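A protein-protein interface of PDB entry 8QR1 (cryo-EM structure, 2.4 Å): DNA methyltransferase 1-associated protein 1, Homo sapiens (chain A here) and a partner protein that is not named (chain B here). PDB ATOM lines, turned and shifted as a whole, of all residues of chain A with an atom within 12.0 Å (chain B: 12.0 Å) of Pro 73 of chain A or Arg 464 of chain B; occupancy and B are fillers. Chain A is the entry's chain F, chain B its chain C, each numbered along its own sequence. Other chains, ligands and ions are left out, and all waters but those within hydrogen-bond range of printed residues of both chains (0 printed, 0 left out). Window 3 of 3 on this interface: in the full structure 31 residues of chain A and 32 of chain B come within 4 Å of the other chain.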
ATOM      1  N   PRO A  69      -8.494 -20.835  -3.789  1.00  0.00           N
ATOM      2  CA  PRO A  69      -7.208 -20.228  -3.475  1.00  0.00           C
ATOM      3  C   PRO A  69      -6.257 -21.256  -2.890  1.00  0.00           C
ATOM      4  O   PRO A  69      -6.689 -22.338  -2.467  1.00  0.00           O
ATOM      5  CB  PRO A  69      -7.570 -19.151  -2.447  1.00  0.00           C
ATOM      6  CG  PRO A  69      -8.756 -19.678  -1.787  1.00  0.00           C
ATOM      7  CD  PRO A  69      -9.535 -20.360  -2.859  1.00  0.00           C
ATOM      8  N   PRO A  70      -4.957 -20.966  -2.847  1.00  0.00           N
ATOM      9  CA  PRO A  70      -4.019 -21.927  -2.270  1.00  0.00           C
ATOM     10  C   PRO A  70      -4.196 -22.057  -0.767  1.00  0.00           C
ATOM     11  O   PRO A  70      -4.921 -21.293  -0.129  1.00  0.00           O
ATOM     12  CB  PRO A  70      -2.653 -21.335  -2.615  1.00  0.00           C
ATOM     13  CG  PRO A  70      -2.898 -19.900  -2.705  1.00  0.00           C
ATOM     14  CD  PRO A  70      -4.254 -19.766  -3.324  1.00  0.00           C
ATOM     15  N   LEU A  71      -3.520 -23.060  -0.213  1.00  0.00           N
ATOM     16  CA  LEU A  71      -3.459 -23.282   1.225  1.00  0.00           C
ATOM     17  C   LEU A  71      -2.095 -22.836   1.727  1.00  0.00           C
ATOM     18  O   LEU A  71      -1.066 -23.339   1.264  1.00  0.00           O
ATOM     19  CB  LEU A  71      -3.694 -24.753   1.556  1.00  0.00           C
ATOM     20  CG  LEU A  71      -4.953 -25.404   0.996  1.00  0.00           C
ATOM     21  CD1 LEU A  71      -4.992 -26.854   1.396  1.00  0.00           C
ATOM     22  CD2 LEU A  71      -6.192 -24.697   1.475  1.00  0.00           C
ATOM     23  N   LEU A  72      -2.091 -21.906   2.675  1.00  0.00           N
ATOM     24  CA  LEU A  72      -0.870 -21.346   3.236  1.00  0.00           C
ATOM     25  C   LEU A  72      -0.509 -22.064   4.536  1.00  0.00           C
ATOM     26  O   LEU A  72      -1.398 -22.568   5.226  1.00  0.00           O
ATOM     27  CB  LEU A  72      -1.039 -19.859   3.514  1.00  0.00           C
ATOM     28  CG  LEU A  72      -0.541 -18.916   2.425  1.00  0.00           C
ATOM     29  CD1 LEU A  72      -1.244 -19.186   1.118  1.00  0.00           C
ATOM     30  CD2 LEU A  72      -0.750 -17.489   2.856  1.00  0.00           C
ATOM     31  N   PRO A  73       0.763 -22.155   4.932  1.00  0.00           N
ATOM     32  CA  PRO A  73       1.062 -22.702   6.257  1.00  0.00           C
ATOM     33  C   PRO A  73       0.593 -21.771   7.363  1.00  0.00           C
ATOM     34  O   PRO A  73       0.534 -20.552   7.198  1.00  0.00           O
ATOM     35  CB  PRO A  73       2.588 -22.837   6.254  1.00  0.00           C
ATOM     36  CG  PRO A  73       2.978 -22.799   4.852  1.00  0.00           C
ATOM     37  CD  PRO A  73       2.002 -21.925   4.172  1.00  0.00           C
ATOM     38  N   SER A  74       0.256 -22.365   8.503  1.00  0.00           N
ATOM     39  CA  SER A  74      -0.057 -21.596   9.696  1.00  0.00           C
ATOM     40  C   SER A  74       0.162 -22.459  10.926  1.00  0.00           C
ATOM     41  O   SER A  74       0.008 -23.682  10.883  1.00  0.00           O
ATOM     42  CB  SER A  74      -1.491 -21.077   9.679  1.00  0.00           C
ATOM     43  OG  SER A  74      -1.656 -19.987  10.564  1.00  0.00           O
ATOM     44  N   ASP A  75       0.518 -21.794  12.022  1.00  0.00           N
ATOM     45  CA  ASP A  75       0.739 -22.433  13.310  1.00  0.00           C
ATOM     46  C   ASP A  75      -0.433 -22.252  14.263  1.00  0.00           C
ATOM     47  O   ASP A  75      -0.654 -23.108  15.127  1.00  0.00           O
ATOM     48  CB  ASP A  75       2.003 -21.868  13.955  1.00  0.00           C
ATOM     49  CG  ASP A  75       3.247 -22.156  13.149  1.00  0.00           C
ATOM     50  OD1 ASP A  75       3.427 -23.316  12.727  1.00  0.00           O
ATOM     51  OD2 ASP A  75       4.046 -21.223  12.933  1.00  0.00           O
ATOM     52  N   THR A  76      -1.192 -21.166  14.115  1.00  0.00           N
ATOM     53  CA  THR A  76      -2.251 -20.788  15.041  1.00  0.00           C
ATOM     54  C   THR A  76      -3.638 -21.165  14.538  1.00  0.00           C
ATOM     55  O   THR A  76      -4.626 -20.560  14.963  1.00  0.00           O
ATOM     56  CB  THR A  76      -2.182 -19.284  15.308  1.00  0.00           C
ATOM     57  OG1 THR A  76      -2.287 -18.577  14.068  1.00  0.00           O
ATOM     58  CG2 THR A  76      -0.875 -18.922  15.971  1.00  0.00           C
ATOM     59  N   GLY A  77      -3.737 -22.148  13.644  1.00  0.00           N
ATOM     60  CA  GLY A  77      -5.037 -22.538  13.129  1.00  0.00           C
ATOM     61  C   GLY A  77      -5.959 -23.100  14.191  1.00  0.00           C
ATOM     62  O   GLY A  77      -7.178 -22.927  14.111  1.00  0.00           O
ATOM     63  N   GLN A  78      -5.395 -23.773  15.195  1.00  0.00           N
ATOM     64  CA  GLN A  78      -6.150 -24.355  16.299  1.00  0.00           C
ATOM     65  C   GLN A  78      -6.200 -23.441  17.521  1.00  0.00           C
ATOM     66  O   GLN A  78      -6.433 -23.927  18.633  1.00  0.00           O
ATOM     67  CB  GLN A  78      -5.550 -25.711  16.699  1.00  0.00           C
ATOM     68  CG  GLN A  78      -5.363 -26.808  15.611  1.00  0.00           C
ATOM     69  CD  GLN A  78      -6.180 -26.632  14.337  1.00  0.00           C
ATOM     70  OE1 GLN A  78      -5.630 -26.618  13.237  1.00  0.00           O
ATOM     71  NE2 GLN A  78      -7.497 -26.569  14.479  1.00  0.00           N
ATOM     72  N   GLY A  79      -5.990 -22.141  17.342  1.00  0.00           N
ATOM     73  CA  GLY A  79      -6.003 -21.191  18.433  1.00  0.00           C
ATOM     74  C   GLY A  79      -4.628 -20.970  19.037  1.00  0.00           C
ATOM     75  O   GLY A  79      -3.724 -21.797  18.940  1.00  0.00           O
ATOM     76  N   VAL A  83      -1.093 -23.502  21.459  1.00  0.00           N
ATOM     77  CA  VAL A  83       0.339 -23.451  21.193  1.00  0.00           C
ATOM     78  C   VAL A  83       1.026 -22.326  21.958  1.00  0.00           C
ATOM     79  O   VAL A  83       2.055 -21.824  21.510  1.00  0.00           O
ATOM     80  CB  VAL A  83       0.619 -23.322  19.682  1.00  0.00           C
ATOM     81  CG1 VAL A  83       0.009 -24.483  18.925  1.00  0.00           C
ATOM     82  CG2 VAL A  83       0.118 -21.990  19.120  1.00  0.00           C
ATOM     83  N   LEU A  87       5.312 -21.559  21.600  1.00  0.00           N
ATOM     84  CA  LEU A  87       5.829 -20.266  21.171  1.00  0.00           C
ATOM     85  C   LEU A  87       6.543 -19.548  22.309  1.00  0.00           C
ATOM     86  O   LEU A  87       7.580 -18.912  22.091  1.00  0.00           O
ATOM     87  CB  LEU A  87       4.691 -19.403  20.631  1.00  0.00           C
ATOM     88  CG  LEU A  87       3.905 -19.957  19.443  1.00  0.00           C
ATOM     89  CD1 LEU A  87       2.672 -19.118  19.192  1.00  0.00           C
ATOM     90  CD2 LEU A  87       4.764 -20.022  18.199  1.00  0.00           C
ATOM     91  N   TRP A  95      16.949 -10.296  12.931  1.00  0.00           N
ATOM     92  CA  TRP A  95      17.145  -9.949  11.534  1.00  0.00           C
ATOM     93  C   TRP A  95      17.626  -8.509  11.437  1.00  0.00           C
ATOM     94  O   TRP A  95      17.471  -7.718  12.370  1.00  0.00           O
ATOM     95  CB  TRP A  95      15.849 -10.125  10.746  1.00  0.00           C
ATOM     96  CG  TRP A  95      15.467 -11.547  10.512  1.00  0.00           C
ATOM     97  CD1 TRP A  95      15.113 -12.462  11.451  1.00  0.00           C
ATOM     98  CD2 TRP A  95      15.395 -12.220   9.253  1.00  0.00           C
ATOM     99  NE1 TRP A  95      14.827 -13.663  10.859  1.00  0.00           N
ATOM    100  CE2 TRP A  95      14.995 -13.539   9.507  1.00  0.00           C
ATOM    101  CE3 TRP A  95      15.634 -11.833   7.934  1.00  0.00           C
ATOM    102  CZ2 TRP A  95      14.827 -14.471   8.497  1.00  0.00           C
ATOM    103  CZ3 TRP A  95      15.467 -12.759   6.936  1.00  0.00           C
ATOM    104  CH2 TRP A  95      15.068 -14.061   7.220  1.00  0.00           C
ATOM    105  N   ARG A 116      19.261 -12.666   8.307  1.00  0.00           N
ATOM    106  CA  ARG A 116      19.611 -12.839   9.708  1.00  0.00           C
ATOM    107  C   ARG A 116      20.971 -12.220   9.997  1.00  0.00           C
ATOM    108  O   ARG A 116      21.885 -12.270   9.171  1.00  0.00           O
ATOM    109  CB  ARG A 116      19.615 -14.319  10.078  1.00  0.00           C
ATOM    110  CG  ARG A 116      18.257 -14.876  10.436  1.00  0.00           C
ATOM    111  CD  ARG A 116      18.318 -16.351  10.755  1.00  0.00           C
ATOM    112  NE  ARG A 116      18.533 -17.166   9.563  1.00  0.00           N
ATOM    113  CZ  ARG A 116      17.583 -17.703   8.804  1.00  0.00           C
ATOM    114  NH1 ARG A 116      16.295 -17.547   9.069  1.00  0.00           N
ATOM    115  NH2 ARG A 116      17.935 -18.417   7.741  1.00  0.00           N
ATOM    116  N   LEU B 445      -4.514 -34.735   3.371  1.00  0.00           N
ATOM    117  CA  LEU B 445      -3.795 -34.109   4.472  1.00  0.00           C
ATOM    118  C   LEU B 445      -3.952 -34.925   5.751  1.00  0.00           C
ATOM    119  O   LEU B 445      -4.972 -35.584   5.970  1.00  0.00           O
ATOM    120  CB  LEU B 445      -4.302 -32.680   4.690  1.00  0.00           C
ATOM    121  CG  LEU B 445      -4.317 -31.764   3.462  1.00  0.00           C
ATOM    122  CD1 LEU B 445      -4.919 -30.418   3.796  1.00  0.00           C
ATOM    123  CD2 LEU B 445      -2.927 -31.582   2.904  1.00  0.00           C
ATOM    124  N   VAL B 447      -4.013 -33.813   8.922  1.00  0.00           N
ATOM    125  CA  VAL B 447      -5.126 -33.239   9.681  1.00  0.00           C
ATOM    126  C   VAL B 447      -6.409 -33.693   8.998  1.00  0.00           C
ATOM    127  O   VAL B 447      -6.420 -33.809   7.755  1.00  0.00           O
ATOM    128  CB  VAL B 447      -5.016 -31.701   9.734  1.00  0.00           C
ATOM    129  CG1 VAL B 447      -6.067 -31.078  10.643  1.00  0.00           C
ATOM    130  CG2 VAL B 447      -3.637 -31.295  10.242  1.00  0.00           C
ATOM    131  N   GLN B 449      -8.915 -32.944   7.402  1.00  0.00           N
ATOM    132  CA  GLN B 449      -9.581 -32.367   6.239  1.00  0.00           C
ATOM    133  C   GLN B 449      -9.237 -33.054   4.918  1.00  0.00           C
ATOM    134  O   GLN B 449      -8.687 -32.415   4.016  1.00  0.00           O
ATOM    135  CB  GLN B 449      -9.264 -30.874   6.118  1.00  0.00           C
ATOM    136  CG  GLN B 449      -9.562 -30.072   7.375  1.00  0.00           C
ATOM    137  CD  GLN B 449      -8.335 -29.695   8.189  1.00  0.00           C
ATOM    138  OE1 GLN B 449      -7.242 -30.228   7.996  1.00  0.00           O
ATOM    139  NE2 GLN B 449      -8.522 -28.764   9.117  1.00  0.00           N
ATOM    140  N   ILE B 452      -8.500 -32.787  -0.803  1.00  0.00           N
ATOM    141  CA  ILE B 452      -8.683 -31.396  -1.209  1.00  0.00           C
ATOM    142  C   ILE B 452      -8.779 -31.263  -2.727  1.00  0.00           C
ATOM    143  O   ILE B 452      -8.725 -30.149  -3.258  1.00  0.00           O
ATOM    144  CB  ILE B 452      -7.555 -30.506  -0.645  1.00  0.00           C
ATOM    145  CG1 ILE B 452      -6.155 -30.938  -1.120  1.00  0.00           C
ATOM    146  CG2 ILE B 452      -7.605 -30.520   0.875  1.00  0.00           C
ATOM    147  CD1 ILE B 452      -5.071 -29.958  -0.778  1.00  0.00           C
ATOM    148  N   ARG B 456      -0.994 -28.924  -6.557  1.00  0.00           N
ATOM    149  CA  ARG B 456       0.459 -28.963  -6.659  1.00  0.00           C
ATOM    150  C   ARG B 456       1.058 -28.519  -5.338  1.00  0.00           C
ATOM    151  O   ARG B 456       0.372 -27.940  -4.497  1.00  0.00           O
ATOM    152  CB  ARG B 456       1.027 -28.027  -7.726  1.00  0.00           C
ATOM    153  CG  ARG B 456       0.207 -27.823  -8.944  1.00  0.00           C
ATOM    154  CD  ARG B 456       0.922 -26.932  -9.941  1.00  0.00           C
ATOM    155  NE  ARG B 456       0.963 -25.547  -9.481  1.00  0.00           N
ATOM    156  CZ  ARG B 456       0.938 -24.464 -10.249  1.00  0.00           C
ATOM    157  NH1 ARG B 456       0.937 -24.535 -11.570  1.00  0.00           N
ATOM    158  NH2 ARG B 456       0.916 -23.267  -9.674  1.00  0.00           N
ATOM    159  N   ARG B 457       2.352 -28.782  -5.185  1.00  0.00           N
ATOM    160  CA  ARG B 457       3.166 -28.181  -4.140  1.00  0.00           C
ATOM    161  C   ARG B 457       4.099 -27.163  -4.775  1.00  0.00           C
ATOM    162  O   ARG B 457       4.793 -27.475  -5.747  1.00  0.00           O
ATOM    163  CB  ARG B 457       3.969 -29.246  -3.401  1.00  0.00           C
ATOM    164  CG  ARG B 457       3.128 -30.219  -2.617  1.00  0.00           C
ATOM    165  CD  ARG B 457       3.990 -31.228  -1.900  1.00  0.00           C
ATOM    166  NE  ARG B 457       4.559 -30.665  -0.678  1.00  0.00           N
ATOM    167  CZ  ARG B 457       5.743 -30.959  -0.153  1.00  0.00           C
ATOM    168  NH1 ARG B 457       6.567 -31.834  -0.711  1.00  0.00           N
ATOM    169  NH2 ARG B 457       6.113 -30.361   0.974  1.00  0.00           N
ATOM    170  N   ARG B 458       4.105 -25.950  -4.230  1.00  0.00           N
ATOM    171  CA  ARG B 458       4.911 -24.853  -4.740  1.00  0.00           C
ATOM    172  C   ARG B 458       5.528 -24.093  -3.579  1.00  0.00           C
ATOM    173  O   ARG B 458       4.861 -23.824  -2.577  1.00  0.00           O
ATOM    174  CB  ARG B 458       4.078 -23.897  -5.597  1.00  0.00           C
ATOM    175  CG  ARG B 458       4.906 -22.987  -6.479  1.00  0.00           C
ATOM    176  CD  ARG B 458       4.097 -21.864  -7.074  1.00  0.00           C
ATOM    177  NE  ARG B 458       3.930 -20.765  -6.125  1.00  0.00           N
ATOM    178  CZ  ARG B 458       2.838 -20.478  -5.425  1.00  0.00           C
ATOM    179  NH1 ARG B 458       1.723 -21.183  -5.530  1.00  0.00           N
ATOM    180  NH2 ARG B 458       2.864 -19.449  -4.587  1.00  0.00           N
ATOM    181  N   VAL B 459       6.802 -23.752  -3.727  1.00  0.00           N
ATOM    182  CA  VAL B 459       7.493 -22.905  -2.764  1.00  0.00           C
ATOM    183  C   VAL B 459       7.226 -21.454  -3.125  1.00  0.00           C
ATOM    184  O   VAL B 459       7.428 -21.040  -4.272  1.00  0.00           O
ATOM    185  CB  VAL B 459       9.000 -23.209  -2.748  1.00  0.00           C
ATOM    186  CG1 VAL B 459       9.698 -22.409  -1.652  1.00  0.00           C
ATOM    187  CG2 VAL B 459       9.235 -24.695  -2.562  1.00  0.00           C
ATOM    188  N   GLY B 460       6.760 -20.681  -2.144  1.00  0.00           N
ATOM    189  CA  GLY B 460       6.522 -19.268  -2.312  1.00  0.00           C
ATOM    190  C   GLY B 460       7.674 -18.430  -1.784  1.00  0.00           C
ATOM    191  O   GLY B 460       8.741 -18.922  -1.427  1.00  0.00           O
ATOM    192  N   ARG B 461       7.433 -17.125  -1.749  1.00  0.00           N
ATOM    193  CA  ARG B 461       8.387 -16.212  -1.146  1.00  0.00           C
ATOM    194  C   ARG B 461       8.504 -16.489   0.347  1.00  0.00           C
ATOM    195  O   ARG B 461       7.539 -16.876   1.009  1.00  0.00           O
ATOM    196  CB  ARG B 461       7.958 -14.767  -1.381  1.00  0.00           C
ATOM    197  CG  ARG B 461       8.350 -14.218  -2.726  1.00  0.00           C
ATOM    198  CD  ARG B 461       7.754 -12.850  -2.965  1.00  0.00           C
ATOM    199  NE  ARG B 461       6.341 -12.910  -3.320  1.00  0.00           N
ATOM    200  CZ  ARG B 461       5.567 -11.857  -3.548  1.00  0.00           C
ATOM    201  NH1 ARG B 461       6.033 -10.620  -3.501  1.00  0.00           N
ATOM    202  NH2 ARG B 461       4.285 -12.049  -3.840  1.00  0.00           N
ATOM    203  N   GLY B 462       9.711 -16.295   0.872  1.00  0.00           N
ATOM    204  CA  GLY B 462       9.970 -16.539   2.274  1.00  0.00           C
ATOM    205  C   GLY B 462      10.230 -17.979   2.647  1.00  0.00           C
ATOM    206  O   GLY B 462      10.266 -18.292   3.840  1.00  0.00           O
ATOM    207  N   GLY B 463      10.418 -18.868   1.675  1.00  0.00           N
ATOM    208  CA  GLY B 463      10.649 -20.265   1.966  1.00  0.00           C
ATOM    209  C   GLY B 463       9.421 -21.051   2.355  1.00  0.00           C
ATOM    210  O   GLY B 463       9.559 -22.183   2.833  1.00  0.00           O
ATOM    211  N   ARG B 464       8.231 -20.498   2.155  1.00  0.00           N
ATOM    212  CA  ARG B 464       7.001 -21.119   2.617  1.00  0.00           C
ATOM    213  C   ARG B 464       6.421 -22.009   1.530  1.00  0.00           C
ATOM    214  O   ARG B 464       6.259 -21.585   0.383  1.00  0.00           O
ATOM    215  CB  ARG B 464       5.986 -20.047   3.016  1.00  0.00           C
ATOM    216  CG  ARG B 464       6.501 -19.045   4.040  1.00  0.00           C
ATOM    217  CD  ARG B 464       5.495 -17.970   4.357  1.00  0.00           C
ATOM    218  NE  ARG B 464       4.597 -18.371   5.440  1.00  0.00           N
ATOM    219  CZ  ARG B 464       3.277 -18.522   5.376  1.00  0.00           C
ATOM    220  NH1 ARG B 464       2.586 -18.291   4.271  1.00  0.00           N
ATOM    221  NH2 ARG B 464       2.626 -18.913   6.464  1.00  0.00           N
ATOM    222  N   VAL B 465       6.103 -23.245   1.902  1.00  0.00           N
ATOM    223  CA  VAL B 465       5.595 -24.250   0.978  1.00  0.00           C
ATOM    224  C   VAL B 465       4.077 -24.200   0.999  1.00  0.00           C
ATOM    225  O   VAL B 465       3.457 -24.412   2.048  1.00  0.00           O
ATOM    226  CB  VAL B 465       6.099 -25.655   1.347  1.00  0.00           C
ATOM    227  CG1 VAL B 465       5.562 -26.679   0.356  1.00  0.00           C
ATOM    228  CG2 VAL B 465       7.623 -25.670   1.409  1.00  0.00           C
ATOM    229  N   LEU B 466       3.485 -23.927  -0.160  1.00  0.00           N
ATOM    230  CA  LEU B 466       2.048 -23.776  -0.321  1.00  0.00           C
ATOM    231  C   LEU B 466       1.497 -24.924  -1.149  1.00  0.00           C
ATOM    232  O   LEU B 466       2.249 -25.671  -1.783  1.00  0.00           O
ATOM    233  CB  LEU B 466       1.697 -22.459  -1.008  1.00  0.00           C
ATOM    234  CG  LEU B 466       2.534 -21.220  -0.693  1.00  0.00           C
ATOM    235  CD1 LEU B 466       1.989 -20.037  -1.438  1.00  0.00           C
ATOM    236  CD2 LEU B 466       2.551 -20.918   0.780  1.00  0.00           C
ATOM    237  N   LEU B 467       0.172 -25.054  -1.125  1.00  0.00           N
ATOM    238  CA  LEU B 467      -0.561 -26.021  -1.934  1.00  0.00           C
ATOM    239  C   LEU B 467      -1.515 -25.265  -2.846  1.00  0.00           C
ATOM    240  O   LEU B 467      -2.516 -24.711  -2.384  1.00  0.00           O
ATOM    241  CB  LEU B 467      -1.334 -27.002  -1.058  1.00  0.00           C
ATOM    242  CG  LEU B 467      -0.622 -28.249  -0.538  1.00  0.00           C
ATOM    243  CD1 LEU B 467      -1.478 -28.926   0.503  1.00  0.00           C
ATOM    244  CD2 LEU B 467      -0.305 -29.214  -1.656  1.00  0.00           C
ATOM    245  N   ASP B 468      -1.209 -25.245  -4.137  1.00  0.00           N
ATOM    246  CA  ASP B 468      -2.153 -24.726  -5.111  1.00  0.00           C
ATOM    247  C   ASP B 468      -3.313 -25.697  -5.263  1.00  0.00           C
ATOM    248  O   ASP B 468      -3.229 -26.859  -4.862  1.00  0.00           O
ATOM    249  CB  ASP B 468      -1.474 -24.511  -6.459  1.00  0.00           C
ATOM    250  CG  ASP B 468      -0.399 -23.455  -6.405  1.00  0.00           C
ATOM    251  OD1 ASP B 468      -0.569 -22.466  -5.664  1.00  0.00           O
ATOM    252  OD2 ASP B 468       0.620 -23.608  -7.109  1.00  0.00           O
ATOM    253  N   ARG B 469      -4.409 -25.206  -5.833  1.00  0.00           N
ATOM    254  CA  ARG B 469      -5.598 -26.011  -6.062  1.00  0.00           C
ATOM    255  C   ARG B 469      -6.241 -25.619  -7.380  1.00  0.00           C
ATOM    256  O   ARG B 469      -6.169 -24.460  -7.798  1.00  0.00           O
ATOM    257  CB  ARG B 469      -6.596 -25.857  -4.921  1.00  0.00           C
ATOM    258  CG  ARG B 469      -6.109 -26.452  -3.621  1.00  0.00           C
ATOM    259  CD  ARG B 469      -7.185 -26.505  -2.571  1.00  0.00           C
ATOM    260  NE  ARG B 469      -7.491 -25.190  -2.027  1.00  0.00           N
ATOM    261  CZ  ARG B 469      -8.547 -24.899  -1.276  1.00  0.00           C
ATOM    262  NH1 ARG B 469      -9.465 -25.806  -0.978  1.00  0.00           N
ATOM    263  NH2 ARG B 469      -8.686 -23.663  -0.812  1.00  0.00           N
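O of Pro 73 of chain A is in hydrogen-bond range of NH2 of Arg 464 of chain B (2.8 Å). The backbone carbonyl oxygen (O) of Leu 467 of chain B is in hydrogen-bond range of the backbone NH (N) of Leu 71 of chain A (2.9 Å). The backbone carbonyl oxygen of Pro 69 of chain A lies within hydrogen-bond range of the guanidinium group of Arg 469 of chain B, at 2.9 Å.
OD2 of Asp 468 of chain B is in salt-bridge range of NH2 of Arg 456 of chain B (2.6 Å). The backbone carbonyl oxygen (O) of Arg 458 of chain B is in hydrogen-bond range of the backbone NH (N) of Leu 466 of chain B, at 2.8 Å. The guanidinium group (NH1) of Arg 458 of chain B is in salt-bridge range of the side-chain carboxylate (OD1) of Asp 468 of chain B, at 2.6 Å.
Pro 70 of chain A touches Leu 467 of chain B. OD1 of Asp 468 of chain B touches CB of Pro 70 of chain A, 3.9 Å away. CD1 of Ile 452 of chain B touches CD1 of Leu 71 of chain A (3.8 Å). Leu 71 of chain A touches Leu 466 of chain B (O to CA, 3.5 Å). Arg 469 of chain B touches Leu 71 of chain A. Leu 72 of chain A touches Arg 464 of chain B (CG to NH1, 3.7 Å). CG of Pro 73 of chain A touches O of Val 465 of chain B, 3.3 Å away. Pro 73 of chain A touches Leu 466 of chain B.
Of the printed residues of chain B, Pro 70 of chain A touches Leu 467 (3.2 Å) and Asp 468 (3.9 Å). Pro 73 of chain A touches just these residues of chain B: Arg 464, Val 465 and Leu 466. No residue of chain B comes within 4 Å of Ser 74 of chain A. No residue of chain A comes within 4 Å of Arg 458 of chain B. No residue of chain A comes within 4 Å of Val 459 of chain B. No residue of chain A comes within 4 Å of Gly 460 of chain B. Val 465 of chain B touches one residue of chain A. Of the printed residues of chain A, Leu 467 of chain B touches Pro 70 (3.2 Å) and Leu 71 (2.9 Å). Of the printed residues of chain A, Arg 469 of chain B touches Pro 69 (2.9 Å) and Leu 71 (3.5 Å). The nearest printed residue of chain A that does not touch Arg 469 of chain B is Pro 70 of chain A (4.5 Å).
Printed residues of chain B that touch a printed residue of chain A: Ile 452, Arg 464, Val 465, Leu 466, Leu 467, Asp 468 and Arg 469. Hydrophobic or aromatic side chains of chain B that line the printed part of chain A: Ile 452 and Leu 466. Hydrophobic or aromatic side chains of chain A within 4 Å of the printed part of chain B: Pro 69, Pro 70, Leu 71, Leu 72 and Pro 73. Along chain A the printed residues that touch a printed residue of chain B span positions 69 to 73.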
